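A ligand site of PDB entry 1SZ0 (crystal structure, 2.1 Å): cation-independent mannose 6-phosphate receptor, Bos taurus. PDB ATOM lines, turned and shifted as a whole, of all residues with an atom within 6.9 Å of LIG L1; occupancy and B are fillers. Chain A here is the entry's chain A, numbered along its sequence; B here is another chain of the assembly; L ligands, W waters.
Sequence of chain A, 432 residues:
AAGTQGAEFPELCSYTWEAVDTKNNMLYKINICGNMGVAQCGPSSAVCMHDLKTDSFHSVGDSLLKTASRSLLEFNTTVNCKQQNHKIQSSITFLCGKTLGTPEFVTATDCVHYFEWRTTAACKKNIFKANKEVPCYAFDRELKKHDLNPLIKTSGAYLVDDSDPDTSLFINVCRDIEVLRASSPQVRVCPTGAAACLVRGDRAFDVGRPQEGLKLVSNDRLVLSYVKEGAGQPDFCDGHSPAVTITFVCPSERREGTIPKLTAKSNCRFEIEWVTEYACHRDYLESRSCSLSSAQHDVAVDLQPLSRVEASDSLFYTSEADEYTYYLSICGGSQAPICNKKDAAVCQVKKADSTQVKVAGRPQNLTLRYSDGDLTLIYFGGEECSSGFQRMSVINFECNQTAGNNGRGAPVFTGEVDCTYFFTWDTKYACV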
ATOM      1  N   LYS A 125       8.483  24.890 -36.440  1.00  0.00           N
ATOM      2  CA  LYS A 125       7.337  24.657 -35.577  1.00  0.00           C
ATOM      3  C   LYS A 125       6.126  25.413 -36.102  1.00  0.00           C
ATOM      4  O   LYS A 125       6.039  26.638 -35.970  1.00  0.00           O
ATOM      5  CB  LYS A 125       7.662  25.110 -34.159  1.00  0.00           C
ATOM      6  CG  LYS A 125       8.752  24.275 -33.497  1.00  0.00           C
ATOM      7  CD  LYS A 125       9.176  24.868 -32.169  1.00  0.00           C
ATOM      8  CE  LYS A 125      10.046  23.888 -31.407  1.00  0.00           C
ATOM      9  NZ  LYS A 125       9.278  22.672 -31.050  1.00  0.00           N
ATOM     10  N   GLU A 323      16.258  35.070 -15.125  1.00  0.00           N
ATOM     11  CA  GLU A 323      17.127  33.952 -15.488  1.00  0.00           C
ATOM     12  C   GLU A 323      18.330  34.343 -16.340  1.00  0.00           C
ATOM     13  O   GLU A 323      19.308  33.581 -16.415  1.00  0.00           O
ATOM     14  CB  GLU A 323      16.329  32.905 -16.259  1.00  0.00           C
ATOM     15  CG  GLU A 323      15.055  32.421 -15.593  1.00  0.00           C
ATOM     16  CD  GLU A 323      14.277  31.472 -16.491  1.00  0.00           C
ATOM     17  OE1 GLU A 323      14.840  30.432 -16.886  1.00  0.00           O
ATOM     18  OE2 GLU A 323      13.101  31.782 -16.800  1.00  0.00           O
ATOM     19  N   TYR A 324      18.282  35.500 -16.988  1.00  0.00           N
ATOM     20  CA  TYR A 324      19.383  35.943 -17.856  1.00  0.00           C
ATOM     21  C   TYR A 324      19.828  37.381 -17.640  1.00  0.00           C
ATOM     22  O   TYR A 324      19.214  38.155 -16.915  1.00  0.00           O
ATOM     23  CB  TYR A 324      18.997  35.797 -19.344  1.00  0.00           C
ATOM     24  CG  TYR A 324      18.456  34.455 -19.762  1.00  0.00           C
ATOM     25  CD1 TYR A 324      17.106  34.140 -19.607  1.00  0.00           C
ATOM     26  CD2 TYR A 324      19.300  33.482 -20.300  1.00  0.00           C
ATOM     27  CE1 TYR A 324      16.612  32.892 -19.959  1.00  0.00           C
ATOM     28  CE2 TYR A 324      18.818  32.233 -20.664  1.00  0.00           C
ATOM     29  CZ  TYR A 324      17.479  31.944 -20.486  1.00  0.00           C
ATOM     30  OH  TYR A 324      17.008  30.693 -20.832  1.00  0.00           O
ATOM     31  N   TYR A 326      21.197  40.673 -20.091  1.00  0.00           N
ATOM     32  CA  TYR A 326      21.288  41.134 -21.467  1.00  0.00           C
ATOM     33  C   TYR A 326      22.292  42.279 -21.639  1.00  0.00           C
ATOM     34  O   TYR A 326      22.196  43.295 -20.967  1.00  0.00           O
ATOM     35  CB  TYR A 326      19.911  41.586 -21.982  1.00  0.00           C
ATOM     36  CG  TYR A 326      18.870  40.495 -21.997  1.00  0.00           C
ATOM     37  CD1 TYR A 326      18.114  40.193 -20.863  1.00  0.00           C
ATOM     38  CD2 TYR A 326      18.651  39.734 -23.148  1.00  0.00           C
ATOM     39  CE1 TYR A 326      17.182  39.166 -20.864  1.00  0.00           C
ATOM     40  CE2 TYR A 326      17.722  38.697 -23.169  1.00  0.00           C
ATOM     41  CZ  TYR A 326      16.988  38.421 -22.023  1.00  0.00           C
ATOM     42  OH  TYR A 326      16.082  37.376 -22.017  1.00  0.00           O
ATOM     43  N   GLN A 348      22.571  37.578 -24.962  1.00  0.00           N
ATOM     44  CA  GLN A 348      21.953  36.972 -23.797  1.00  0.00           C
ATOM     45  C   GLN A 348      22.831  35.908 -23.169  1.00  0.00           C
ATOM     46  O   GLN A 348      23.350  35.035 -23.864  1.00  0.00           O
ATOM     47  CB  GLN A 348      20.605  36.364 -24.167  1.00  0.00           C
ATOM     48  CG  GLN A 348      19.923  35.667 -22.992  1.00  0.00           C
ATOM     49  CD  GLN A 348      18.766  34.810 -23.427  1.00  0.00           C
ATOM     50  OE1 GLN A 348      17.613  35.093 -23.111  1.00  0.00           O
ATOM     51  NE2 GLN A 348      19.072  33.737 -24.151  1.00  0.00           N
ATOM     52  N   LYS A 350      22.862  33.096 -19.891  1.00  0.00           N
ATOM     53  CA  LYS A 350      22.108  32.479 -18.806  1.00  0.00           C
ATOM     54  C   LYS A 350      22.893  32.574 -17.511  1.00  0.00           C
ATOM     55  O   LYS A 350      24.072  32.204 -17.463  1.00  0.00           O
ATOM     56  CB  LYS A 350      21.814  30.999 -19.125  1.00  0.00           C
ATOM     57  CG  LYS A 350      20.648  30.440 -18.315  1.00  0.00           C
ATOM     58  CD  LYS A 350      20.679  28.928 -18.258  1.00  0.00           C
ATOM     59  CE  LYS A 350      20.465  28.289 -19.609  1.00  0.00           C
ATOM     60  NZ  LYS A 350      20.680  26.808 -19.571  1.00  0.00           N
ATOM     61  N   GLN A 356      26.181  29.616 -21.527  1.00  0.00           N
ATOM     62  CA  GLN A 356      25.185  29.847 -22.555  1.00  0.00           C
ATOM     63  C   GLN A 356      25.092  31.324 -22.946  1.00  0.00           C
ATOM     64  O   GLN A 356      24.575  32.148 -22.201  1.00  0.00           O
ATOM     65  CB  GLN A 356      23.814  29.347 -22.072  1.00  0.00           C
ATOM     66  CG  GLN A 356      22.910  28.940 -23.200  1.00  0.00           C
ATOM     67  CD  GLN A 356      21.624  28.322 -22.705  1.00  0.00           C
ATOM     68  OE1 GLN A 356      21.638  27.359 -21.936  1.00  0.00           O
ATOM     69  NE2 GLN A 356      20.499  28.862 -23.151  1.00  0.00           N
ATOM     70  N   LYS A 358      23.755  33.640 -26.059  1.00  0.00           N
ATOM     71  CA  LYS A 358      22.951  33.669 -27.278  1.00  0.00           C
ATOM     72  C   LYS A 358      22.863  35.055 -27.904  1.00  0.00           C
ATOM     73  O   LYS A 358      22.686  36.051 -27.209  1.00  0.00           O
ATOM     74  CB  LYS A 358      21.545  33.163 -26.961  1.00  0.00           C
ATOM     75  CG  LYS A 358      21.491  31.719 -26.478  1.00  0.00           C
ATOM     76  CD  LYS A 358      21.869  30.759 -27.604  1.00  0.00           C
ATOM     77  CE  LYS A 358      21.701  29.311 -27.166  1.00  0.00           C
ATOM     78  NZ  LYS A 358      22.049  28.375 -28.257  1.00  0.00           N
ATOM     79  N   GLU A 384      18.948  31.311 -34.117  1.00  0.00           N
ATOM     80  CA  GLU A 384      17.680  30.597 -34.237  1.00  0.00           C
ATOM     81  C   GLU A 384      17.256  29.869 -32.974  1.00  0.00           C
ATOM     82  O   GLU A 384      18.078  29.417 -32.198  1.00  0.00           O
ATOM     83  CB  GLU A 384      17.750  29.556 -35.357  1.00  0.00           C
ATOM     84  CG  GLU A 384      17.658  30.114 -36.768  1.00  0.00           C
ATOM     85  CD  GLU A 384      17.634  29.015 -37.813  1.00  0.00           C
ATOM     86  OE1 GLU A 384      17.529  29.336 -39.023  1.00  0.00           O
ATOM     87  OE2 GLU A 384      17.710  27.828 -37.438  1.00  0.00           O
ATOM     88  N   CYS A 385      15.949  29.785 -32.786  1.00  0.00           N
ATOM     89  CA  CYS A 385      15.387  29.050 -31.665  1.00  0.00           C
ATOM     90  C   CYS A 385      14.878  27.774 -32.342  1.00  0.00           C
ATOM     91  O   CYS A 385      14.837  27.710 -33.574  1.00  0.00           O
ATOM     92  CB  CYS A 385      14.264  29.869 -31.001  1.00  0.00           C
ATOM     93  SG  CYS A 385      14.964  31.186 -29.939  1.00  0.00           S
ATOM     94  N   SER A 386      14.504  26.757 -31.563  1.00  0.00           N
ATOM     95  CA  SER A 386      14.034  25.500 -32.138  1.00  0.00           C
ATOM     96  C   SER A 386      12.927  25.725 -33.171  1.00  0.00           C
ATOM     97  O   SER A 386      12.782  24.952 -34.118  1.00  0.00           O
ATOM     98  CB  SER A 386      13.522  24.564 -31.047  1.00  0.00           C
ATOM     99  OG  SER A 386      12.507  25.188 -30.271  1.00  0.00           O
ATOM    100  N   SER A 387      12.152  26.787 -32.967  1.00  0.00           N
ATOM    101  CA  SER A 387      11.073  27.109 -33.898  1.00  0.00           C
ATOM    102  C   SER A 387      11.617  27.452 -35.280  1.00  0.00           C
ATOM    103  O   SER A 387      10.927  27.296 -36.275  1.00  0.00           O
ATOM    104  CB  SER A 387      10.264  28.294 -33.363  1.00  0.00           C
ATOM    105  OG  SER A 387      11.107  29.412 -33.168  1.00  0.00           O
ATOM    106  N   GLY A 388      12.863  27.910 -35.319  1.00  0.00           N
ATOM    107  CA  GLY A 388      13.461  28.304 -36.588  1.00  0.00           C
ATOM    108  C   GLY A 388      13.627  29.812 -36.619  1.00  0.00           C
ATOM    109  O   GLY A 388      14.373  30.374 -37.441  1.00  0.00           O
ATOM    110  N   ARG A 391      16.562  34.983 -33.275  1.00  0.00           N
ATOM    111  CA  ARG A 391      16.253  35.854 -32.161  1.00  0.00           C
ATOM    112  C   ARG A 391      16.214  37.311 -32.634  1.00  0.00           C
ATOM    113  O   ARG A 391      16.920  37.717 -33.566  1.00  0.00           O
ATOM    114  CB  ARG A 391      17.263  35.661 -31.038  1.00  0.00           C
ATOM    115  CG  ARG A 391      17.025  34.394 -30.196  1.00  0.00           C
ATOM    116  CD  ARG A 391      18.139  34.210 -29.183  1.00  0.00           C
ATOM    117  NE  ARG A 391      17.911  33.100 -28.256  1.00  0.00           N
ATOM    118  CZ  ARG A 391      18.061  31.814 -28.560  1.00  0.00           C
ATOM    119  NH1 ARG A 391      18.444  31.439 -29.768  1.00  0.00           N
ATOM    120  NH2 ARG A 391      17.851  30.894 -27.628  1.00  0.00           N
ATOM    121  N   GLU A 416      10.179  38.614 -22.650  1.00  0.00           N
ATOM    122  CA  GLU A 416      10.396  37.894 -23.883  1.00  0.00           C
ATOM    123  C   GLU A 416       9.085  37.294 -24.367  1.00  0.00           C
ATOM    124  O   GLU A 416       8.176  37.054 -23.581  1.00  0.00           O
ATOM    125  CB  GLU A 416      11.426  36.765 -23.708  1.00  0.00           C
ATOM    126  CG  GLU A 416      11.392  35.791 -24.878  1.00  0.00           C
ATOM    127  CD  GLU A 416      12.190  34.524 -24.644  1.00  0.00           C
ATOM    128  OE1 GLU A 416      12.599  34.271 -23.488  1.00  0.00           O
ATOM    129  OE2 GLU A 416      12.405  33.772 -25.609  1.00  0.00           O
ATOM    130  N   ASP A 418       8.457  34.395 -27.343  1.00  0.00           N
ATOM    131  CA  ASP A 418       8.904  33.494 -28.413  1.00  0.00           C
ATOM    132  C   ASP A 418      10.117  33.948 -29.184  1.00  0.00           C
ATOM    133  O   ASP A 418      10.078  34.071 -30.417  1.00  0.00           O
ATOM    134  CB  ASP A 418       7.761  33.222 -29.381  1.00  0.00           C
ATOM    135  CG  ASP A 418       6.532  32.647 -28.678  1.00  0.00           C
ATOM    136  OD1 ASP A 418       6.730  31.820 -27.758  1.00  0.00           O
ATOM    137  OD2 ASP A 418       5.395  33.010 -29.048  1.00  0.00           O
ATOM    138  N   CYS A 419      11.202  34.179 -28.455  1.00  0.00           N
ATOM    139  CA  CYS A 419      12.473  34.589 -29.035  1.00  0.00           C
ATOM    140  C   CYS A 419      12.568  35.999 -29.627  1.00  0.00           C
ATOM    141  O   CYS A 419      13.420  36.288 -30.480  1.00  0.00           O
ATOM    142  CB  CYS A 419      12.940  33.498 -29.993  1.00  0.00           C
ATOM    143  SG  CYS A 419      13.407  32.050 -28.989  1.00  0.00           S
ATOM    144  N   TYR A 421      12.862  39.633 -27.866  1.00  0.00           N
ATOM    145  CA  TYR A 421      13.096  40.271 -26.583  1.00  0.00           C
ATOM    146  C   TYR A 421      12.791  41.771 -26.623  1.00  0.00           C
ATOM    147  O   TYR A 421      13.254  42.488 -27.508  1.00  0.00           O
ATOM    148  CB  TYR A 421      14.539  40.014 -26.160  1.00  0.00           C
ATOM    149  CG  TYR A 421      14.933  38.544 -26.272  1.00  0.00           C
ATOM    150  CD1 TYR A 421      15.264  37.974 -27.506  1.00  0.00           C
ATOM    151  CD2 TYR A 421      14.967  37.717 -25.135  1.00  0.00           C
ATOM    152  CE1 TYR A 421      15.611  36.616 -27.606  1.00  0.00           C
ATOM    153  CE2 TYR A 421      15.315  36.375 -25.226  1.00  0.00           C
ATOM    154  CZ  TYR A 421      15.636  35.824 -26.462  1.00  0.00           C
ATOM    155  OH  TYR A 421      15.984  34.482 -26.554  1.00  0.00           O
ATOM    156  N   GLU B 323      17.130  15.699 -31.296  1.00  0.00           N
ATOM    157  CA  GLU B 323      17.727  17.029 -31.433  1.00  0.00           C
ATOM    158  C   GLU B 323      19.224  17.091 -31.224  1.00  0.00           C
ATOM    159  O   GLU B 323      19.819  18.167 -31.326  1.00  0.00           O
ATOM    160  CB  GLU B 323      17.096  18.018 -30.459  1.00  0.00           C
ATOM    161  CG  GLU B 323      15.696  18.472 -30.801  1.00  0.00           C
ATOM    162  CD  GLU B 323      15.340  19.745 -30.048  1.00  0.00           C
ATOM    163  OE1 GLU B 323      15.943  20.808 -30.349  1.00  0.00           O
ATOM    164  OE2 GLU B 323      14.467  19.690 -29.158  1.00  0.00           O
ATOM    165  N   TYR B 324      19.845  15.960 -30.908  1.00  0.00           N
ATOM    166  CA  TYR B 324      21.280  15.962 -30.674  1.00  0.00           C
ATOM    167  C   TYR B 324      21.922  14.707 -31.218  1.00  0.00           C
ATOM    168  O   TYR B 324      21.248  13.763 -31.620  1.00  0.00           O
ATOM    169  CB  TYR B 324      21.607  16.023 -29.177  1.00  0.00           C
ATOM    170  CG  TYR B 324      20.963  17.144 -28.421  1.00  0.00           C
ATOM    171  CD1 TYR B 324      19.629  17.050 -27.996  1.00  0.00           C
ATOM    172  CD2 TYR B 324      21.670  18.307 -28.117  1.00  0.00           C
ATOM    173  CE1 TYR B 324      19.029  18.089 -27.289  1.00  0.00           C
ATOM    174  CE2 TYR B 324      21.083  19.347 -27.414  1.00  0.00           C
ATOM    175  CZ  TYR B 324      19.763  19.238 -27.000  1.00  0.00           C
ATOM    176  OH  TYR B 324      19.183  20.272 -26.297  1.00  0.00           O
ATOM    177  N   LYS B 350      24.337  19.649 -30.306  1.00  0.00           N
ATOM    178  CA  LYS B 350      23.049  20.112 -30.814  1.00  0.00           C
ATOM    179  C   LYS B 350      23.104  20.086 -32.347  1.00  0.00           C
ATOM    180  O   LYS B 350      24.094  20.522 -32.935  1.00  0.00           O
ATOM    181  CB  LYS B 350      22.759  21.521 -30.309  1.00  0.00           C
ATOM    182  CG  LYS B 350      21.322  21.974 -30.486  1.00  0.00           C
ATOM    183  CD  LYS B 350      21.002  23.220 -29.653  1.00  0.00           C
ATOM    184  CE  LYS B 350      19.504  23.393 -29.485  1.00  0.00           C
ATOM    185  NZ  LYS B 350      19.110  24.458 -28.509  1.00  0.00           N
HETATM  186  C1  LIG L   1      17.240  29.920 -24.335  1.00  0.00           C
HETATM  187  C2  LIG L   1      16.930  31.442 -24.221  1.00  0.00           C
HETATM  188  C3  LIG L   1      15.378  31.699 -24.127  1.00  0.00           C
HETATM  189  C4  LIG L   1      14.707  31.103 -25.394  1.00  0.00           C
HETATM  190  C5  LIG L   1      15.008  29.577 -25.432  1.00  0.00           C
HETATM  191  C6  LIG L   1      14.445  28.885 -26.647  1.00  0.00           C
HETATM  192  O1  LIG L   1      16.848  29.217 -23.115  1.00  0.00           O
HETATM  193  O2  LIG L   1      17.398  32.046 -25.432  1.00  0.00           O
HETATM  194  O3  LIG L   1      15.122  33.101 -24.037  1.00  0.00           O
HETATM  195  O4  LIG L   1      13.293  31.311 -25.346  1.00  0.00           O
HETATM  196  O5  LIG L   1      16.473  29.349 -25.458  1.00  0.00           O
HETATM  197  O6  LIG L   1      14.743  27.497 -26.572  1.00  0.00           O
HETATM  198  P1  LIG L   1      14.306  26.513 -27.714  1.00  0.00           P
HETATM  199  O7  LIG L   1      14.761  25.013 -27.346  1.00  0.00           O
HETATM  200  O8  LIG L   1      15.086  26.955 -29.036  1.00  0.00           O
HETATM  201  O9  LIG L   1      12.728  26.594 -27.970  1.00  0.00           O
HETATM  202  C1  LG2 L   2      20.874  21.486 -23.193  1.00  0.00           C
HETATM  203  C2  LG2 L   2      20.997  19.936 -23.361  1.00  0.00           C
HETATM  204  C3  LG2 L   2      19.712  19.205 -22.806  1.00  0.00           C
HETATM  205  C4  LG2 L   2      19.533  19.570 -21.322  1.00  0.00           C
HETATM  206  C5  LG2 L   2      19.340  21.108 -21.229  1.00  0.00           C
HETATM  207  C6  LG2 L   2      19.193  21.596 -19.817  1.00  0.00           C
HETATM  208  O1  LG2 L   2      19.802  22.005 -24.013  1.00  0.00           O
HETATM  209  O2  LG2 L   2      22.109  19.526 -22.559  1.00  0.00           O
HETATM  210  O3  LG2 L   2      19.866  17.798 -22.954  1.00  0.00           O
HETATM  211  O4  LG2 L   2      18.368  18.920 -20.789  1.00  0.00           O
HETATM  212  O5  LG2 L   2      20.538  21.785 -21.796  1.00  0.00           O
HETATM  213  O6  LG2 L   2      18.991  22.999 -19.854  1.00  0.00           O
HETATM  214  P1  LG2 L   2      18.812  23.815 -18.533  1.00  0.00           P
HETATM  215  O7  LG2 L   2      18.556  25.378 -18.909  1.00  0.00           O
HETATM  216  O8  LG2 L   2      20.174  23.728 -17.723  1.00  0.00           O
HETATM  217  O9  LG2 L   2      17.611  23.236 -17.638  1.00  0.00           O
HETATM  218  O   HOH W   1      11.362  27.728 -30.057  1.00  0.00           O
HETATM  219  O   HOH W   2      10.899  27.328 -26.346  1.00  0.00           O
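Residues that only touch LIG L1: Gln 356 and Cys 385.
Water W1 lies within hydrogen-bond range of an oxygen (O9) of LIG L1 (2.7 Å), the side-chain hydroxyl of Ser 386 (2.8 Å) and the backbone NH of Ser 387 (3.2 Å).
The guanidinium group (NE) of Arg 391 is in hydrogen-bond range of the side-chain hydroxyl (OH) of Tyr 421 (2.9 Å). SG of Cys 385 lies close to NH1 of Arg 391, 3.5 Å away. The guanidinium group (NH1) of Arg 391 lies within hydrogen-bond range of the backbone carbonyl oxygen (O) of Glu 384, 3.2 Å away. The backbone NH (N) of Cys 419 lies within hydrogen-bond range of the side-chain carboxylate (OE2) of Glu 416 (3.1 Å). O of Gln 348 sits at hydrogen-bond distance from N of Lys 358 (2.6 Å). The side-chain amide oxygen (OE1) of Gln 348 lies within hydrogen-bond range of the side-chain hydroxyl (OH) of Tyr 326. SG of Cys 385 forms a disulfide with SG of Cys 419. The side-chain amino group of Lys 350 of chain A sits at hydrogen-bond distance from the side-chain amide oxygen of Gln 356 (2.6 Å).
An oxygen (O2) of LIG L1 is in hydrogen-bond range of the guanidinium group (NH2) of Arg 391 (2.5 Å). O8 of LIG L1 sits at hydrogen-bond distance from N of Ser 386, at 2.6 Å. O9 of LIG L1 lies within hydrogen-bond range of OG of Ser 386 (2.7 Å). OE2 of Glu 416 is in hydrogen-bond range of O4 of LIG L1. The side-chain amide nitrogen of Gln 348 is in hydrogen-bond range of an oxygen (O2) of LIG L1, 2.7 Å away. The side-chain hydroxyl of Tyr 324 of chain A sits at hydrogen-bond distance from an oxygen (O1) of LIG L1. The side-chain hydroxyl (OH) of Tyr 421 is in hydrogen-bond range of an oxygen (O3) of LIG L1, 3.0 Å away. SG of Cys 419 sits at hydrogen-bond distance from O4 of LIG L1 (3.7 Å). NZ of Lys 350 of chain A is in salt-bridge range of O7 of LG2 L2 (2.6 Å).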
